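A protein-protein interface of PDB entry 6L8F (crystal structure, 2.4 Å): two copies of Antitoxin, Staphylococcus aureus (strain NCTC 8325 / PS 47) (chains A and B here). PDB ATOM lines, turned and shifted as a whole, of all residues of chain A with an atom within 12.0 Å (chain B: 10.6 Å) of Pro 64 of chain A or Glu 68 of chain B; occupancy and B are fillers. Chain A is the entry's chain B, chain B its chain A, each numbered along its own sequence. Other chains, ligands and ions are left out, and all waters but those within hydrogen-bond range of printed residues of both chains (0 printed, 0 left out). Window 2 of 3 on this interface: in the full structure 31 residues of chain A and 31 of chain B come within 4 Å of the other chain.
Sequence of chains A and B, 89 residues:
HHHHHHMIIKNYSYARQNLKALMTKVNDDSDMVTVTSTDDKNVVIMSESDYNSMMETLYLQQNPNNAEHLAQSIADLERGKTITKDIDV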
ATOM      1  N   THR A  57      12.279  27.754  -8.379  1.00  0.00           N
ATOM      2  CA  THR A  57      13.502  27.289  -9.031  1.00  0.00           C
ATOM      3  C   THR A  57      13.858  28.156 -10.229  1.00  0.00           C
ATOM      4  O   THR A  57      15.026  28.528 -10.401  1.00  0.00           O
ATOM      5  CB  THR A  57      13.350  25.831  -9.459  1.00  0.00           C
ATOM      6  OG1 THR A  57      13.006  25.034  -8.317  1.00  0.00           O
ATOM      7  CG2 THR A  57      14.652  25.306 -10.049  1.00  0.00           C
ATOM      8  N   LEU A  58      12.859  28.510 -11.053  1.00  0.00           N
ATOM      9  CA  LEU A  58      13.113  29.381 -12.197  1.00  0.00           C
ATOM     10  C   LEU A  58      13.553  30.756 -11.740  1.00  0.00           C
ATOM     11  O   LEU A  58      14.424  31.363 -12.370  1.00  0.00           O
ATOM     12  CB  LEU A  58      11.872  29.506 -13.079  1.00  0.00           C
ATOM     13  CG  LEU A  58      11.556  28.351 -14.032  1.00  0.00           C
ATOM     14  CD1 LEU A  58      10.142  28.459 -14.525  1.00  0.00           C
ATOM     15  CD2 LEU A  58      12.515  28.318 -15.214  1.00  0.00           C
ATOM     16  N   TYR A  59      12.976  31.242 -10.623  1.00  0.00           N
ATOM     17  CA  TYR A  59      13.393  32.518 -10.045  1.00  0.00           C
ATOM     18  C   TYR A  59      14.866  32.496  -9.643  1.00  0.00           C
ATOM     19  O   TYR A  59      15.616  33.434  -9.944  1.00  0.00           O
ATOM     20  CB  TYR A  59      12.528  32.867  -8.827  1.00  0.00           C
ATOM     21  CG  TYR A  59      13.061  34.084  -8.113  1.00  0.00           C
ATOM     22  CD1 TYR A  59      13.144  35.310  -8.773  1.00  0.00           C
ATOM     23  CD2 TYR A  59      13.522  34.010  -6.798  1.00  0.00           C
ATOM     24  CE1 TYR A  59      13.656  36.429  -8.142  1.00  0.00           C
ATOM     25  CE2 TYR A  59      14.030  35.124  -6.158  1.00  0.00           C
ATOM     26  CZ  TYR A  59      14.096  36.330  -6.837  1.00  0.00           C
ATOM     27  OH  TYR A  59      14.606  37.447  -6.216  1.00  0.00           O
ATOM     28  N   LEU A  60      15.299  31.427  -8.974  1.00  0.00           N
ATOM     29  CA  LEU A  60      16.687  31.342  -8.538  1.00  0.00           C
ATOM     30  C   LEU A  60      17.652  31.157  -9.711  1.00  0.00           C
ATOM     31  O   LEU A  60      18.786  31.646  -9.656  1.00  0.00           O
ATOM     32  CB  LEU A  60      16.826  30.211  -7.518  1.00  0.00           C
ATOM     33  CG  LEU A  60      16.158  30.502  -6.167  1.00  0.00           C
ATOM     34  CD1 LEU A  60      16.150  29.290  -5.264  1.00  0.00           C
ATOM     35  CD2 LEU A  60      16.850  31.667  -5.459  1.00  0.00           C
ATOM     36  N   GLN A  61      17.219  30.505 -10.787  1.00  0.00           N
ATOM     37  CA  GLN A  61      18.097  30.247 -11.921  1.00  0.00           C
ATOM     38  C   GLN A  61      18.009  31.305 -13.015  1.00  0.00           C
ATOM     39  O   GLN A  61      18.822  31.272 -13.946  1.00  0.00           O
ATOM     40  CB  GLN A  61      17.797  28.865 -12.504  1.00  0.00           C
ATOM     41  CG  GLN A  61      18.267  27.734 -11.589  1.00  0.00           C
ATOM     42  CD  GLN A  61      17.829  26.371 -12.071  1.00  0.00           C
ATOM     43  OE1 GLN A  61      16.976  26.249 -12.954  1.00  0.00           O
ATOM     44  NE2 GLN A  61      18.413  25.329 -11.493  1.00  0.00           N
ATOM     45  N   GLN A  62      17.079  32.259 -12.889  1.00  0.00           N
ATOM     46  CA  GLN A  62      16.792  33.247 -13.932  1.00  0.00           C
ATOM     47  C   GLN A  62      17.991  34.131 -14.262  1.00  0.00           C
ATOM     48  O   GLN A  62      18.135  34.581 -15.404  1.00  0.00           O
ATOM     49  CB  GLN A  62      15.620  34.113 -13.469  1.00  0.00           C
ATOM     50  CG  GLN A  62      15.090  35.101 -14.459  1.00  0.00           C
ATOM     51  CD  GLN A  62      14.022  35.964 -13.847  1.00  0.00           C
ATOM     52  OE1 GLN A  62      13.970  36.114 -12.625  1.00  0.00           O
ATOM     53  NE2 GLN A  62      13.151  36.532 -14.688  1.00  0.00           N
ATOM     54  N   ASN A  63      18.840  34.407 -13.287  1.00  0.00           N
ATOM     55  CA  ASN A  63      20.052  35.157 -13.559  1.00  0.00           C
ATOM     56  C   ASN A  63      21.237  34.216 -13.505  1.00  0.00           C
ATOM     57  O   ASN A  63      21.368  33.463 -12.524  1.00  0.00           O
ATOM     58  CB  ASN A  63      20.242  36.289 -12.559  1.00  0.00           C
ATOM     59  CG  ASN A  63      19.225  37.407 -12.749  1.00  0.00           C
ATOM     60  OD1 ASN A  63      18.177  37.443 -12.091  1.00  0.00           O
ATOM     61  ND2 ASN A  63      19.530  38.327 -13.657  1.00  0.00           N
ATOM     62  N   PRO A  64      22.089  34.226 -14.542  1.00  0.00           N
ATOM     63  CA  PRO A  64      23.177  33.238 -14.620  1.00  0.00           C
ATOM     64  C   PRO A  64      24.209  33.368 -13.517  1.00  0.00           C
ATOM     65  O   PRO A  64      24.778  32.349 -13.105  1.00  0.00           O
ATOM     66  CB  PRO A  64      23.793  33.516 -15.999  1.00  0.00           C
ATOM     67  CG  PRO A  64      23.455  34.966 -16.262  1.00  0.00           C
ATOM     68  CD  PRO A  64      22.075  35.126 -15.710  1.00  0.00           C
ATOM     69  N   ASN A  65      24.469  34.585 -13.030  1.00  0.00           N
ATOM     70  CA  ASN A  65      25.313  34.753 -11.852  1.00  0.00           C
ATOM     71  C   ASN A  65      24.716  34.067 -10.633  1.00  0.00           C
ATOM     72  O   ASN A  65      25.460  33.525  -9.808  1.00  0.00           O
ATOM     73  CB  ASN A  65      25.523  36.233 -11.547  1.00  0.00           C
ATOM     74  CG  ASN A  65      26.446  36.904 -12.543  1.00  0.00           C
ATOM     75  OD1 ASN A  65      27.202  36.235 -13.232  1.00  0.00           O
ATOM     76  ND2 ASN A  65      26.396  38.232 -12.615  1.00  0.00           N
ATOM     77  N   ASN A  66      23.384  34.050 -10.511  1.00  0.00           N
ATOM     78  CA  ASN A  66      22.804  33.401  -9.343  1.00  0.00           C
ATOM     79  C   ASN A  66      22.798  31.892  -9.490  1.00  0.00           C
ATOM     80  O   ASN A  66      23.024  31.182  -8.503  1.00  0.00           O
ATOM     81  CB  ASN A  66      21.386  33.892  -9.068  1.00  0.00           C
ATOM     82  CG  ASN A  66      20.941  33.546  -7.666  1.00  0.00           C
ATOM     83  OD1 ASN A  66      21.584  33.954  -6.702  1.00  0.00           O
ATOM     84  ND2 ASN A  66      19.880  32.767  -7.540  1.00  0.00           N
ATOM     85  N   ALA A  67      22.539  31.395 -10.711  1.00  0.00           N
ATOM     86  CA  ALA A  67      22.607  29.959 -10.969  1.00  0.00           C
ATOM     87  C   ALA A  67      24.004  29.429 -10.702  1.00  0.00           C
ATOM     88  O   ALA A  67      24.170  28.347 -10.125  1.00  0.00           O
ATOM     89  CB  ALA A  67      22.200  29.663 -12.417  1.00  0.00           C
ATOM     90  N   GLU A  68      25.018  30.207 -11.084  1.00  0.00           N
ATOM     91  CA  GLU A  68      26.404  29.835 -10.827  1.00  0.00           C
ATOM     92  C   GLU A  68      26.715  29.885  -9.343  1.00  0.00           C
ATOM     93  O   GLU A  68      27.407  29.003  -8.821  1.00  0.00           O
ATOM     94  CB  GLU A  68      27.334  30.775 -11.590  1.00  0.00           C
ATOM     95  CG  GLU A  68      28.765  30.332 -11.652  1.00  0.00           C
ATOM     96  CD  GLU A  68      28.962  29.151 -12.578  1.00  0.00           C
ATOM     97  OE1 GLU A  68      29.311  28.060 -12.070  1.00  0.00           O
ATOM     98  OE2 GLU A  68      28.766  29.316 -13.809  1.00  0.00           O
ATOM     99  N   HIS A  69      26.214  30.921  -8.657  1.00  0.00           N
ATOM    100  CA  HIS A  69      26.427  31.084  -7.223  1.00  0.00           C
ATOM    101  C   HIS A  69      25.829  29.924  -6.440  1.00  0.00           C
ATOM    102  O   HIS A  69      26.465  29.401  -5.518  1.00  0.00           O
ATOM    103  CB  HIS A  69      25.829  32.417  -6.771  1.00  0.00           C
ATOM    104  CG  HIS A  69      25.452  32.467  -5.323  1.00  0.00           C
ATOM    105  ND1 HIS A  69      26.349  32.225  -4.309  1.00  0.00           N
ATOM    106  CD2 HIS A  69      24.270  32.758  -4.723  1.00  0.00           C
ATOM    107  CE1 HIS A  69      25.736  32.355  -3.140  1.00  0.00           C
ATOM    108  NE2 HIS A  69      24.477  32.681  -3.365  1.00  0.00           N
ATOM    109  N   LEU A  70      24.629  29.485  -6.822  1.00  0.00           N
ATOM    110  CA  LEU A  70      24.003  28.351  -6.150  1.00  0.00           C
ATOM    111  C   LEU A  70      24.762  27.056  -6.404  1.00  0.00           C
ATOM    112  O   LEU A  70      24.982  26.280  -5.472  1.00  0.00           O
ATOM    113  CB  LEU A  70      22.546  28.224  -6.593  1.00  0.00           C
ATOM    114  CG  LEU A  70      21.663  29.330  -6.006  1.00  0.00           C
ATOM    115  CD1 LEU A  70      20.217  29.170  -6.431  1.00  0.00           C
ATOM    116  CD2 LEU A  70      21.783  29.344  -4.484  1.00  0.00           C
ATOM    117  N   ALA A  71      25.200  26.823  -7.651  1.00  0.00           N
ATOM    118  CA  ALA A  71      25.857  25.563  -7.995  1.00  0.00           C
ATOM    119  C   ALA A  71      27.223  25.457  -7.338  1.00  0.00           C
ATOM    120  O   ALA A  71      27.596  24.382  -6.857  1.00  0.00           O
ATOM    121  CB  ALA A  71      25.983  25.416  -9.515  1.00  0.00           C
ATOM    122  N   GLN A  72      27.970  26.566  -7.286  1.00  0.00           N
ATOM    123  CA  GLN A  72      29.257  26.571  -6.593  1.00  0.00           C
ATOM    124  C   GLN A  72      29.081  26.358  -5.093  1.00  0.00           C
ATOM    125  O   GLN A  72      29.881  25.656  -4.462  1.00  0.00           O
ATOM    126  CB  GLN A  72      29.994  27.886  -6.857  1.00  0.00           C
ATOM    127  CG  GLN A  72      30.467  28.049  -8.291  1.00  0.00           C
ATOM    128  CD  GLN A  72      30.860  29.483  -8.636  1.00  0.00           C
ATOM    129  OE1 GLN A  72      30.650  30.418  -7.851  1.00  0.00           O
ATOM    130  NE2 GLN A  72      31.443  29.656  -9.812  1.00  0.00           N
ATOM    131  N   SER A  73      28.036  26.955  -4.511  1.00  0.00           N
ATOM    132  CA  SER A  73      27.822  26.871  -3.071  1.00  0.00           C
ATOM    133  C   SER A  73      27.382  25.475  -2.651  1.00  0.00           C
ATOM    134  O   SER A  73      27.846  24.956  -1.625  1.00  0.00           O
ATOM    135  CB  SER A  73      26.779  27.901  -2.643  1.00  0.00           C
ATOM    136  OG  SER A  73      27.293  29.208  -2.786  1.00  0.00           O
ATOM    137  N   THR B  57      12.185  25.333 -20.257  1.00  0.00           N
ATOM    138  CA  THR B  57      13.023  26.379 -19.684  1.00  0.00           C
ATOM    139  C   THR B  57      13.843  25.852 -18.510  1.00  0.00           C
ATOM    140  O   THR B  57      15.051  26.078 -18.454  1.00  0.00           O
ATOM    141  CB  THR B  57      12.154  27.564 -19.261  1.00  0.00           C
ATOM    142  OG1 THR B  57      11.329  27.957 -20.364  1.00  0.00           O
ATOM    143  CG2 THR B  57      13.024  28.746 -18.853  1.00  0.00           C
ATOM    144  N   TYR B  59      14.734  22.732 -18.024  1.00  0.00           N
ATOM    145  CA  TYR B  59      15.727  21.819 -18.586  1.00  0.00           C
ATOM    146  C   TYR B  59      16.949  22.573 -19.095  1.00  0.00           C
ATOM    147  O   TYR B  59      18.087  22.153 -18.863  1.00  0.00           O
ATOM    148  CB  TYR B  59      15.104  20.993 -19.715  1.00  0.00           C
ATOM    149  CG  TYR B  59      16.116  20.229 -20.531  1.00  0.00           C
ATOM    150  CD1 TYR B  59      16.906  19.254 -19.938  1.00  0.00           C
ATOM    151  CD2 TYR B  59      16.282  20.472 -21.897  1.00  0.00           C
ATOM    152  CE1 TYR B  59      17.840  18.544 -20.664  1.00  0.00           C
ATOM    153  CE2 TYR B  59      17.224  19.750 -22.647  1.00  0.00           C
ATOM    154  CZ  TYR B  59      17.996  18.790 -22.013  1.00  0.00           C
ATOM    155  OH  TYR B  59      18.935  18.076 -22.708  1.00  0.00           O
ATOM    156  N   LEU B  60      16.734  23.717 -19.741  1.00  0.00           N
ATOM    157  CA  LEU B  60      17.848  24.489 -20.269  1.00  0.00           C
ATOM    158  C   LEU B  60      18.621  25.226 -19.183  1.00  0.00           C
ATOM    159  O   LEU B  60      19.816  25.485 -19.366  1.00  0.00           O
ATOM    160  CB  LEU B  60      17.340  25.468 -21.328  1.00  0.00           C
ATOM    161  CG  LEU B  60      16.824  24.730 -22.568  1.00  0.00           C
ATOM    162  CD1 LEU B  60      16.025  25.654 -23.478  1.00  0.00           C
ATOM    163  CD2 LEU B  60      17.997  24.104 -23.311  1.00  0.00           C
ATOM    164  N   GLN B  61      17.970  25.575 -18.056  1.00  0.00           N
ATOM    165  CA  GLN B  61      18.648  26.273 -16.966  1.00  0.00           C
ATOM    166  C   GLN B  61      19.343  25.339 -15.987  1.00  0.00           C
ATOM    167  O   GLN B  61      20.114  25.822 -15.155  1.00  0.00           O
ATOM    168  CB  GLN B  61      17.680  27.128 -16.120  1.00  0.00           C
ATOM    169  CG  GLN B  61      16.732  28.105 -16.797  1.00  0.00           C
ATOM    170  CD  GLN B  61      17.348  29.399 -17.244  1.00  0.00           C
ATOM    171  OE1 GLN B  61      18.377  29.418 -17.913  1.00  0.00           O
ATOM    172  NE2 GLN B  61      16.697  30.501 -16.905  1.00  0.00           N
ATOM    173  N   GLN B  62      19.068  24.034 -16.019  1.00  0.00           N
ATOM    174  CA  GLN B  62      19.410  23.215 -14.860  1.00  0.00           C
ATOM    175  C   GLN B  62      20.885  22.869 -14.766  1.00  0.00           C
ATOM    176  O   GLN B  62      21.308  22.360 -13.723  1.00  0.00           O
ATOM    177  CB  GLN B  62      18.608  21.923 -14.847  1.00  0.00           C
ATOM    178  CG  GLN B  62      19.160  20.865 -15.743  1.00  0.00           C
ATOM    179  CD  GLN B  62      18.154  19.787 -16.010  1.00  0.00           C
ATOM    180  OE1 GLN B  62      17.009  19.855 -15.547  1.00  0.00           O
ATOM    181  NE2 GLN B  62      18.564  18.783 -16.765  1.00  0.00           N
ATOM    182  N   ASN B  63      21.667  23.104 -15.817  1.00  0.00           N
ATOM    183  CA  ASN B  63      23.110  23.064 -15.686  1.00  0.00           C
ATOM    184  C   ASN B  63      23.650  24.467 -15.839  1.00  0.00           C
ATOM    185  O   ASN B  63      23.280  25.156 -16.797  1.00  0.00           O
ATOM    186  CB  ASN B  63      23.737  22.137 -16.713  1.00  0.00           C
ATOM    187  CG  ASN B  63      23.499  20.680 -16.369  1.00  0.00           C
ATOM    188  OD1 ASN B  63      24.346  20.027 -15.730  1.00  0.00           O
ATOM    189  ND2 ASN B  63      22.323  20.164 -16.751  1.00  0.00           N
ATOM    190  N   PRO B  64      24.480  24.931 -14.895  1.00  0.00           N
ATOM    191  CA  PRO B  64      24.920  26.335 -14.927  1.00  0.00           C
ATOM    192  C   PRO B  64      25.787  26.666 -16.125  1.00  0.00           C
ATOM    193  O   PRO B  64      25.721  27.802 -16.609  1.00  0.00           O
ATOM    194  CB  PRO B  64      25.695  26.491 -13.609  1.00  0.00           C
ATOM    195  CG  PRO B  64      26.203  25.095 -13.317  1.00  0.00           C
ATOM    196  CD  PRO B  64      25.074  24.188 -13.769  1.00  0.00           C
ATOM    197  N   ASN B  65      26.576  25.708 -16.626  1.00  0.00           N
ATOM    198  CA  ASN B  65      27.318  25.932 -17.864  1.00  0.00           C
ATOM    199  C   ASN B  65      26.381  26.163 -19.044  1.00  0.00           C
ATOM    200  O   ASN B  65      26.721  26.929 -19.953  1.00  0.00           O
ATOM    201  CB  ASN B  65      28.248  24.752 -18.166  1.00  0.00           C
ATOM    202  CG  ASN B  65      29.411  24.654 -17.186  1.00  0.00           C
ATOM    203  OD1 ASN B  65      29.827  25.648 -16.603  1.00  0.00           O
ATOM    204  ND2 ASN B  65      29.940  23.449 -17.007  1.00  0.00           N
ATOM    205  N   ASN B  66      25.189  25.548 -19.045  1.00  0.00           N
ATOM    206  CA  ASN B  66      24.278  25.808 -20.166  1.00  0.00           C
ATOM    207  C   ASN B  66      23.473  27.085 -19.975  1.00  0.00           C
ATOM    208  O   ASN B  66      23.156  27.756 -20.965  1.00  0.00           O
ATOM    209  CB  ASN B  66      23.310  24.647 -20.406  1.00  0.00           C
ATOM    210  CG  ASN B  66      22.643  24.742 -21.765  1.00  0.00           C
ATOM    211  OD1 ASN B  66      23.312  24.655 -22.797  1.00  0.00           O
ATOM    212  ND2 ASN B  66      21.335  24.933 -21.779  1.00  0.00           N
ATOM    213  N   ALA B  67      23.104  27.413 -18.725  1.00  0.00           N
ATOM    214  CA  ALA B  67      22.435  28.687 -18.467  1.00  0.00           C
ATOM    215  C   ALA B  67      23.347  29.845 -18.828  1.00  0.00           C
ATOM    216  O   ALA B  67      22.904  30.839 -19.417  1.00  0.00           O
ATOM    217  CB  ALA B  67      22.003  28.791 -17.000  1.00  0.00           C
ATOM    218  N   GLU B  68      24.633  29.704 -18.517  1.00  0.00           N
ATOM    219  CA  GLU B  68      25.623  30.720 -18.846  1.00  0.00           C
ATOM    220  C   GLU B  68      25.844  30.803 -20.351  1.00  0.00           C
ATOM    221  O   GLU B  68      25.964  31.903 -20.904  1.00  0.00           O
ATOM    222  CB  GLU B  68      26.929  30.406 -18.113  1.00  0.00           C
ATOM    223  CG  GLU B  68      27.996  31.475 -18.207  1.00  0.00           C
ATOM    224  CD  GLU B  68      27.632  32.749 -17.451  1.00  0.00           C
ATOM    225  OE1 GLU B  68      27.291  32.657 -16.246  1.00  0.00           O
ATOM    226  OE2 GLU B  68      27.685  33.842 -18.062  1.00  0.00           O
ATOM    227  N   HIS B  69      25.877  29.648 -21.027  1.00  0.00           N
ATOM    228  CA  HIS B  69      26.055  29.621 -22.475  1.00  0.00           C
ATOM    229  C   HIS B  69      24.876  30.272 -23.183  1.00  0.00           C
ATOM    230  O   HIS B  69      25.064  31.039 -24.132  1.00  0.00           O
ATOM    231  CB  HIS B  69      26.258  28.173 -22.932  1.00  0.00           C
ATOM    232  CG  HIS B  69      25.776  27.876 -24.321  1.00  0.00           C
ATOM    233  ND1 HIS B  69      26.337  28.443 -25.446  1.00  0.00           N
ATOM    234  CD2 HIS B  69      24.807  27.040 -24.766  1.00  0.00           C
ATOM    235  CE1 HIS B  69      25.721  27.984 -26.523  1.00  0.00           C
ATOM    236  NE2 HIS B  69      24.793  27.128 -26.139  1.00  0.00           N
ATOM    237  N   LEU B  70      23.659  30.025 -22.695  1.00  0.00           N
ATOM    238  CA  LEU B  70      22.489  30.667 -23.282  1.00  0.00           C
ATOM    239  C   LEU B  70      22.483  32.171 -23.025  1.00  0.00           C
ATOM    240  O   LEU B  70      22.158  32.948 -23.929  1.00  0.00           O
ATOM    241  CB  LEU B  70      21.213  30.022 -22.750  1.00  0.00           C
ATOM    242  CG  LEU B  70      20.876  28.645 -23.319  1.00  0.00           C
ATOM    243  CD1 LEU B  70      19.646  28.079 -22.639  1.00  0.00           C
ATOM    244  CD2 LEU B  70      20.681  28.695 -24.843  1.00  0.00           C
ATOM    245  N   ALA B  71      22.846  32.596 -21.805  1.00  0.00           N
ATOM    246  CA  ALA B  71      22.874  34.021 -21.482  1.00  0.00           C
ATOM    247  C   ALA B  71      23.905  34.757 -22.323  1.00  0.00           C
ATOM    248  O   ALA B  71      23.607  35.825 -22.870  1.00  0.00           O
ATOM    249  CB  ALA B  71      23.158  34.229 -19.988  1.00  0.00           C
ATOM    250  N   GLN B  72      25.109  34.183 -22.457  1.00  0.00           N
ATOM    251  CA  GLN B  72      26.164  34.783 -23.270  1.00  0.00           C
ATOM    252  C   GLN B  72      25.787  34.841 -24.742  1.00  0.00           C
ATOM    253  O   GLN B  72      26.117  35.813 -25.430  1.00  0.00           O
ATOM    254  CB  GLN B  72      27.458  33.992 -23.106  1.00  0.00           C
ATOM    255  CG  GLN B  72      28.124  34.228 -21.768  1.00  0.00           C
ATOM    256  CD  GLN B  72      29.176  33.186 -21.438  1.00  0.00           C
ATOM    257  OE1 GLN B  72      29.447  32.275 -22.228  1.00  0.00           O
ATOM    258  NE2 GLN B  72      29.780  33.321 -20.266  1.00  0.00           N
ATOM    259  N   SER B  73      25.111  33.803 -25.242  1.00  0.00           N
ATOM    260  CA  SER B  73      24.764  33.747 -26.657  1.00  0.00           C
ATOM    261  C   SER B  73      23.645  34.718 -26.989  1.00  0.00           C
ATOM    262  O   SER B  73      23.683  35.375 -28.036  1.00  0.00           O
ATOM    263  CB  SER B  73      24.357  32.327 -27.039  1.00  0.00           C
ATOM    264  OG  SER B  73      25.477  31.465 -26.985  1.00  0.00           O
ATOM    265  N   ILE B  74      22.637  34.804 -26.115  1.00  0.00           N
ATOM    266  CA  ILE B  74      21.538  35.746 -26.301  1.00  0.00           C
ATOM    267  C   ILE B  74      22.048  37.180 -26.214  1.00  0.00           C
ATOM    268  O   ILE B  74      21.638  38.045 -26.998  1.00  0.00           O
ATOM    269  CB  ILE B  74      20.435  35.447 -25.271  1.00  0.00           C
ATOM    270  CG1 ILE B  74      19.641  34.225 -25.720  1.00  0.00           C
ATOM    271  CG2 ILE B  74      19.516  36.645 -25.028  1.00  0.00           C
ATOM    272  CD1 ILE B  74      18.778  33.633 -24.631  1.00  0.00           C
ATOM    273  N   ALA B  75      22.998  37.428 -25.301  1.00  0.00           N
ATOM    274  CA  ALA B  75      23.666  38.725 -25.209  1.00  0.00           C
ATOM    275  C   ALA B  75      24.416  39.069 -26.491  1.00  0.00           C
ATOM    276  O   ALA B  75      24.314  40.194 -26.991  1.00  0.00           O
ATOM    277  CB  ALA B  75      24.629  38.725 -24.027  1.00  0.00           C
ATOM    278  N   ASP B  76      25.175  38.111 -27.036  1.00  0.00           N
ATOM    279  CA  ASP B  76      25.945  38.367 -28.254  1.00  0.00           C
ATOM    280  C   ASP B  76      25.031  38.642 -29.446  1.00  0.00           C
ATOM    281  O   ASP B  76      25.301  39.549 -30.238  1.00  0.00           O
ATOM    282  CB  ASP B  76      26.865  37.185 -28.547  1.00  0.00           C
ATOM    283  CG  ASP B  76      28.057  37.133 -27.613  1.00  0.00           C
ATOM    284  OD1 ASP B  76      28.431  38.186 -27.059  1.00  0.00           O
ATOM    285  OD2 ASP B  76      28.623  36.039 -27.437  1.00  0.00           O
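Thr 57 of chain A touches none of the printed residues of chain B. Of the printed residues of chain B, Leu 58 of chain A touches Thr 57 (3.7 Å). Of the printed residues of chain B, Gln 61 of chain A touches Gln 61. No residue of chain B comes within 4 Å of Asn 63 of chain A. Of chain B, only Glu 68 (3.6 Å) and Ala 71 (3.8 Å) come within 4 Å of Pro 64 of chain A. No residue of chain B comes within 4 Å of Ala 67 of chain A. No residue of chain B comes within 4 Å of Glu 68 of chain A. Printed residues of chain B within 4 Å of Ala 71 of chain A: Pro 64. Gln 72 of chain A touches none of the printed residues of chain B. Pro 64 of chain B touches just one residue of chain A: Ala 71. No residue of chain A comes within 4 Å of Asn 65 of chain B. No residue of chain A comes within 4 Å of Ala 67 of chain B. Glu 68 of chain B touches one residue of chain A. No residue of chain A comes within 4 Å of His 69 of chain B. No residue of chain A comes within 4 Å of Leu 70 of chain B. No residue of chain A comes within 4 Å of Gln 72 of chain B. The nearest residue of chain B that does not touch Pro 64 of chain A is Ala 67 of chain B (4.4 Å).
Gln 61 of chain B touches its own counterpart, Gln 61 of chain A. Pro 64 of chain A touches Glu 68 of chain B, but with the chains exchanged Glu 68 of chain A does not touch Pro 64 of chain B (4.2 Å). Pro 64 of chain A touches Ala 71 of chain B, and with the chains exchanged Ala 71 of chain A touches Pro 64 of chain B.
Of the 17 printed residues of chain A, 4 touch a printed residue of chain B. Printed residues of chain A that touch a printed residue of chain B: Leu 58, Gln 61, Pro 64 and Ala 71. Hydrophobic or aromatic side chains of chain A within 4 Å of the printed part of chain B: Leu 58, Pro 64 and Ala 71. Along chain A the printed residues that touch a printed residue of chain B span positions 58 to 71. Of the 19 printed residues of chain B, 5 touch a printed residue of chain A. Printed residues of chain B that touch a printed residue of chain A: Thr 57, Gln 61, Pro 64, Glu 68 and Ala 71. Hydrophobic or aromatic side chains of chain B that line the printed part of chain A: Pro 64 and Ala 71.
Among the printed residues, pairs that only touch across the chains: Gln 61 of chain A with Gln 61 of chain B, Pro 64 of chain A with Glu 68 of chain B, Leu 58 of chain A with Thr 57 of chain B, Pro 64 of chain A with Ala 71 of chain B and Ala 71 of chain A with Pro 64 of chain B.
OE2 of Glu 68 of chain B is in hydrogen-bond range of NE2 of Gln 72 of chain B (3.1 Å).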
